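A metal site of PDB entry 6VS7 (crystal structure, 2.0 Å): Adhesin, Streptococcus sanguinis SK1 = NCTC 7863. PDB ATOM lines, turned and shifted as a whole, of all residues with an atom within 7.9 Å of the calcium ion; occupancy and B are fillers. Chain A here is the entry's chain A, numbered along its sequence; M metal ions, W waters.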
ATOM      1  N   THR A   1     -26.402  18.695 -26.863  1.00  0.00           N
ATOM      2  CA  THR A   1     -25.020  19.149 -26.835  1.00  0.00           C
ATOM      3  C   THR A   1     -24.899  20.554 -26.247  1.00  0.00           C
ATOM      4  O   THR A   1     -25.891  21.246 -26.034  1.00  0.00           O
ATOM      5  CB  THR A   1     -24.386  19.183 -28.242  1.00  0.00           C
ATOM      6  OG1 THR A   1     -25.208  19.953 -29.135  1.00  0.00           O
ATOM      7  CG2 THR A   1     -24.195  17.768 -28.786  1.00  0.00           C
ATOM      8  N   ASP A   2     -23.649  20.955 -26.044  1.00  0.00           N
ATOM      9  CA  ASP A   2     -23.305  22.231 -25.444  1.00  0.00           C
ATOM     10  C   ASP A   2     -23.380  23.354 -26.470  1.00  0.00           C
ATOM     11  O   ASP A   2     -22.643  23.340 -27.468  1.00  0.00           O
ATOM     12  CB  ASP A   2     -21.902  22.127 -24.854  1.00  0.00           C
ATOM     13  CG  ASP A   2     -21.573  23.236 -23.887  1.00  0.00           C
ATOM     14  OD1 ASP A   2     -22.031  24.385 -24.080  1.00  0.00           O
ATOM     15  OD2 ASP A   2     -20.820  22.928 -22.932  1.00  0.00           O
ATOM     16  N   THR A   3     -24.249  24.348 -26.246  1.00  0.00           N
ATOM     17  CA  THR A   3     -24.318  25.534 -27.093  1.00  0.00           C
ATOM     18  C   THR A   3     -24.037  26.805 -26.298  1.00  0.00           C
ATOM     19  O   THR A   3     -24.346  27.904 -26.759  1.00  0.00           O
ATOM     20  CB  THR A   3     -25.674  25.619 -27.785  1.00  0.00           C
ATOM     21  OG1 THR A   3     -26.711  25.755 -26.803  1.00  0.00           O
ATOM     22  CG2 THR A   3     -25.922  24.352 -28.591  1.00  0.00           C
ATOM     23  N   THR A   4     -23.447  26.674 -25.110  1.00  0.00           N
ATOM     24  CA  THR A   4     -23.297  27.763 -24.174  1.00  0.00           C
ATOM     25  C   THR A   4     -21.822  28.000 -23.895  1.00  0.00           C
ATOM     26  O   THR A   4     -21.110  27.060 -23.528  1.00  0.00           O
ATOM     27  CB  THR A   4     -24.041  27.427 -22.868  1.00  0.00           C
ATOM     28  OG1 THR A   4     -25.409  27.122 -23.176  1.00  0.00           O
ATOM     29  CG2 THR A   4     -23.999  28.599 -21.891  1.00  0.00           C
ATOM     30  N   PRO A   5     -21.334  29.230 -24.063  1.00  0.00           N
ATOM     31  CA  PRO A   5     -19.907  29.504 -23.841  1.00  0.00           C
ATOM     32  C   PRO A   5     -19.612  29.555 -22.361  1.00  0.00           C
ATOM     33  O   PRO A   5     -20.537  29.632 -21.539  1.00  0.00           O
ATOM     34  CB  PRO A   5     -19.724  30.880 -24.491  1.00  0.00           C
ATOM     35  CG  PRO A   5     -21.057  31.539 -24.269  1.00  0.00           C
ATOM     36  CD  PRO A   5     -22.096  30.449 -24.398  1.00  0.00           C
ATOM     37  N   PRO A   6     -18.350  29.522 -21.964  1.00  0.00           N
ATOM     38  CA  PRO A   6     -18.027  29.529 -20.537  1.00  0.00           C
ATOM     39  C   PRO A   6     -18.408  30.844 -19.871  1.00  0.00           C
ATOM     40  O   PRO A   6     -18.686  31.849 -20.526  1.00  0.00           O
ATOM     41  CB  PRO A   6     -16.507  29.318 -20.504  1.00  0.00           C
ATOM     42  CG  PRO A   6     -16.143  28.816 -21.870  1.00  0.00           C
ATOM     43  CD  PRO A   6     -17.138  29.414 -22.808  1.00  0.00           C
ATOM     44  N   THR A   7     -18.419  30.817 -18.546  1.00  0.00           N
ATOM     45  CA  THR A   7     -18.648  32.003 -17.734  1.00  0.00           C
ATOM     46  C   THR A   7     -17.326  32.537 -17.215  1.00  0.00           C
ATOM     47  O   THR A   7     -16.550  31.800 -16.592  1.00  0.00           O
ATOM     48  CB  THR A   7     -19.578  31.667 -16.573  1.00  0.00           C
ATOM     49  OG1 THR A   7     -20.864  31.307 -17.093  1.00  0.00           O
ATOM     50  CG2 THR A   7     -19.717  32.842 -15.635  1.00  0.00           C
ATOM     51  N   THR A  29     -15.389  29.115 -15.845  1.00  0.00           N
ATOM     52  CA  THR A  29     -16.143  27.880 -15.611  1.00  0.00           C
ATOM     53  C   THR A  29     -17.050  27.552 -16.772  1.00  0.00           C
ATOM     54  O   THR A  29     -17.382  28.401 -17.504  1.00  0.00           O
ATOM     55  CB  THR A  29     -17.065  27.963 -14.406  1.00  0.00           C
ATOM     56  OG1 THR A  29     -18.117  28.847 -14.701  1.00  0.00           O
ATOM     57  CG2 THR A  29     -16.362  28.429 -13.158  1.00  0.00           C
ATOM     58  N   ASP A  30     -17.482  26.303 -16.881  1.00  0.00           N
ATOM     59  CA  ASP A  30     -18.340  25.830 -17.955  1.00  0.00           C
ATOM     60  C   ASP A  30     -19.040  24.571 -17.507  1.00  0.00           C
ATOM     61  O   ASP A  30     -18.500  23.785 -16.798  1.00  0.00           O
ATOM     62  CB  ASP A  30     -17.570  25.660 -19.243  1.00  0.00           C
ATOM     63  CG  ASP A  30     -18.456  25.511 -20.421  1.00  0.00           C
ATOM     64  OD1 ASP A  30     -18.839  26.504 -20.983  1.00  0.00           O
ATOM     65  OD2 ASP A  30     -18.770  24.404 -20.807  1.00  0.00           O
ATOM     66  N   ASP A  31     -20.281  24.416 -17.956  1.00  0.00           N
ATOM     67  CA  ASP A  31     -21.111  23.271 -17.608  1.00  0.00           C
ATOM     68  C   ASP A  31     -20.391  21.931 -17.845  1.00  0.00           C
ATOM     69  O   ASP A  31     -20.432  21.087 -17.028  1.00  0.00           O
ATOM     70  CB  ASP A  31     -22.491  23.330 -18.259  1.00  0.00           C
ATOM     71  CG  ASP A  31     -23.486  24.217 -17.509  1.00  0.00           C
ATOM     72  OD1 ASP A  31     -23.263  24.616 -16.383  1.00  0.00           O
ATOM     73  OD2 ASP A  31     -24.535  24.569 -18.067  1.00  0.00           O
ATOM     74  N   SER A  32     -19.697  21.793 -18.967  1.00  0.00           N
ATOM     75  CA  SER A  32     -18.911  20.630 -19.290  1.00  0.00           C
ATOM     76  C   SER A  32     -17.743  20.319 -18.350  1.00  0.00           C
ATOM     77  O   SER A  32     -17.274  19.215 -18.321  1.00  0.00           O
ATOM     78  CB  SER A  32     -18.358  20.800 -20.666  1.00  0.00           C
ATOM     79  OG  SER A  32     -17.358  21.762 -20.674  1.00  0.00           O
ATOM     80  N   GLY A  33     -17.244  21.332 -17.650  1.00  0.00           N
ATOM     81  CA  GLY A  33     -16.133  21.242 -16.771  1.00  0.00           C
ATOM     82  C   GLY A  33     -14.855  21.419 -17.540  1.00  0.00           C
ATOM     83  O   GLY A  33     -13.838  21.224 -17.012  1.00  0.00           O
ATOM     84  N   ARG A  34     -14.969  21.765 -18.806  1.00  0.00           N
ATOM     85  CA  ARG A  34     -13.802  21.989 -19.618  1.00  0.00           C
ATOM     86  C   ARG A  34     -13.772  23.248 -20.469  1.00  0.00           C
ATOM     87  O   ARG A  34     -14.664  23.504 -21.203  1.00  0.00           O
ATOM     88  CB  ARG A  34     -13.534  20.789 -20.529  1.00  0.00           C
ATOM     89  CG  ARG A  34     -12.367  20.977 -21.481  1.00  0.00           C
ATOM     90  CD  ARG A  34     -12.045  19.758 -22.285  1.00  0.00           C
ATOM     91  NE  ARG A  34     -10.957  19.934 -23.207  1.00  0.00           N
ATOM     92  CZ  ARG A  34     -10.385  18.938 -23.834  1.00  0.00           C
ATOM     93  NH1 ARG A  34     -10.792  17.736 -23.654  1.00  0.00           N
ATOM     94  NH2 ARG A  34      -9.406  19.151 -24.652  1.00  0.00           N
ATOM     95  N   VAL A  35     -12.694  24.002 -20.348  1.00  0.00           N
ATOM     96  CA  VAL A  35     -12.459  25.169 -21.158  1.00  0.00           C
ATOM     97  C   VAL A  35     -11.175  24.979 -21.944  1.00  0.00           C
ATOM     98  O   VAL A  35     -10.173  24.659 -21.401  1.00  0.00           O
ATOM     99  CB  VAL A  35     -12.428  26.476 -20.346  1.00  0.00           C
ATOM    100  CG1 VAL A  35     -11.786  27.603 -21.137  1.00  0.00           C
ATOM    101  CG2 VAL A  35     -13.805  26.794 -19.866  1.00  0.00           C
ATOM    102  N   GLU A 103     -13.521  29.848 -24.588  1.00  0.00           N
ATOM    103  CA  GLU A 103     -14.111  28.945 -25.562  1.00  0.00           C
ATOM    104  C   GLU A 103     -14.087  27.529 -25.010  1.00  0.00           C
ATOM    105  O   GLU A 103     -13.034  27.057 -24.551  1.00  0.00           O
ATOM    106  CB  GLU A 103     -13.346  29.008 -26.889  1.00  0.00           C
ATOM    107  CG  GLU A 103     -13.910  28.137 -28.001  1.00  0.00           C
ATOM    108  CD  GLU A 103     -13.168  28.325 -29.318  1.00  0.00           C
ATOM    109  OE1 GLU A 103     -12.683  27.317 -29.870  1.00  0.00           O
ATOM    110  OE2 GLU A 103     -13.078  29.484 -29.798  1.00  0.00           O
ATOM    111  N   ASP A 104     -15.232  26.848 -25.031  1.00  0.00           N
ATOM    112  CA  ASP A 104     -15.287  25.509 -24.449  1.00  0.00           C
ATOM    113  C   ASP A 104     -14.844  24.472 -25.487  1.00  0.00           C
ATOM    114  O   ASP A 104     -14.476  24.809 -26.611  1.00  0.00           O
ATOM    115  CB  ASP A 104     -16.688  25.224 -23.881  1.00  0.00           C
ATOM    116  CG  ASP A 104     -17.787  25.301 -24.935  1.00  0.00           C
ATOM    117  OD1 ASP A 104     -17.474  25.233 -26.149  1.00  0.00           O
ATOM    118  OD2 ASP A 104     -18.977  25.410 -24.547  1.00  0.00           O
ATOM    119  N   ALA A 105     -14.900  23.188 -25.117  1.00  0.00           N
ATOM    120  CA  ALA A 105     -14.468  22.150 -26.056  1.00  0.00           C
ATOM    121  C   ALA A 105     -15.441  21.989 -27.222  1.00  0.00           C
ATOM    122  O   ALA A 105     -15.044  21.489 -28.280  1.00  0.00           O
ATOM    123  CB  ALA A 105     -14.286  20.820 -25.337  1.00  0.00           C
ATOM    124  N   ALA A 106     -16.687  22.413 -27.066  1.00  0.00           N
ATOM    125  CA  ALA A 106     -17.656  22.332 -28.148  1.00  0.00           C
ATOM    126  C   ALA A 106     -17.545  23.496 -29.126  1.00  0.00           C
ATOM    127  O   ALA A 106     -18.315  23.563 -30.088  1.00  0.00           O
ATOM    128  CB  ALA A 106     -19.083  22.261 -27.579  1.00  0.00           C
ATOM    129  N   GLY A 107     -16.599  24.413 -28.891  1.00  0.00           N
ATOM    130  CA  GLY A 107     -16.373  25.540 -29.762  1.00  0.00           C
ATOM    131  C   GLY A 107     -17.218  26.761 -29.458  1.00  0.00           C
ATOM    132  O   GLY A 107     -17.314  27.656 -30.299  1.00  0.00           O
ATOM    133  N   ASN A 108     -17.859  26.836 -28.293  1.00  0.00           N
ATOM    134  CA  ASN A 108     -18.659  27.998 -27.943  1.00  0.00           C
ATOM    135  C   ASN A 108     -17.726  29.026 -27.296  1.00  0.00           C
ATOM    136  O   ASN A 108     -17.273  28.816 -26.165  1.00  0.00           O
ATOM    137  CB  ASN A 108     -19.786  27.621 -26.987  1.00  0.00           C
ATOM    138  CG  ASN A 108     -20.665  26.539 -27.537  1.00  0.00           C
ATOM    139  OD1 ASN A 108     -21.293  26.715 -28.572  1.00  0.00           O
ATOM    140  ND2 ASN A 108     -20.744  25.424 -26.837  1.00  0.00           N
HETATM  141 CA    CA M   1     -20.317  25.096 -22.520  1.00  0.00          CA
HETATM  142  O   HOH W   1     -21.703  25.008 -21.081  1.00  0.00           O
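The side-chain amide nitrogen (ND2) of Asn 108 lies within hydrogen-bond range of the backbone carbonyl oxygen (O) of Asp 2, 2.9 Å away. The side-chain carboxylate (OD2) of Asp 30 sits close to the side-chain hydroxyl (OG) of Ser 32. The side-chain carboxylate (OD1) of Asp 104 lies within hydrogen-bond range of the backbone NH (N) of Ala 106, at 3.1 Å. N of Gly 107 lies within hydrogen-bond range of OD1 of Asp 104 (3.0 Å). The backbone NH (N) of Asn 108 sits at hydrogen-bond distance from the side-chain carboxylate (OD1) of Asp 104 (2.7 Å). N of Thr 4 sits close to ND2 of Asn 108 (3.4 Å).
The calcium ion is bound by water W1 (2.0 Å), the side-chain carboxylate (OD2) of Asp 2 (2.3 Å), the backbone carbonyl oxygen (O) of Thr 4 (2.3 Å), the side-chain carboxylate (OD2) of Asp 30 (2.4 Å), the side-chain carboxylate (OD1) of Asp 2 (2.4 Å), the side-chain carboxylate (OD2) of Asp 104 (2.5 Å) and the side-chain carboxylate (OD1) of Asp 30 (2.6 Å). The calcium ion has seven donor atoms within binding distance.
Of the 20 residues printed, 4 come within 4 Å of the calcium ion.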
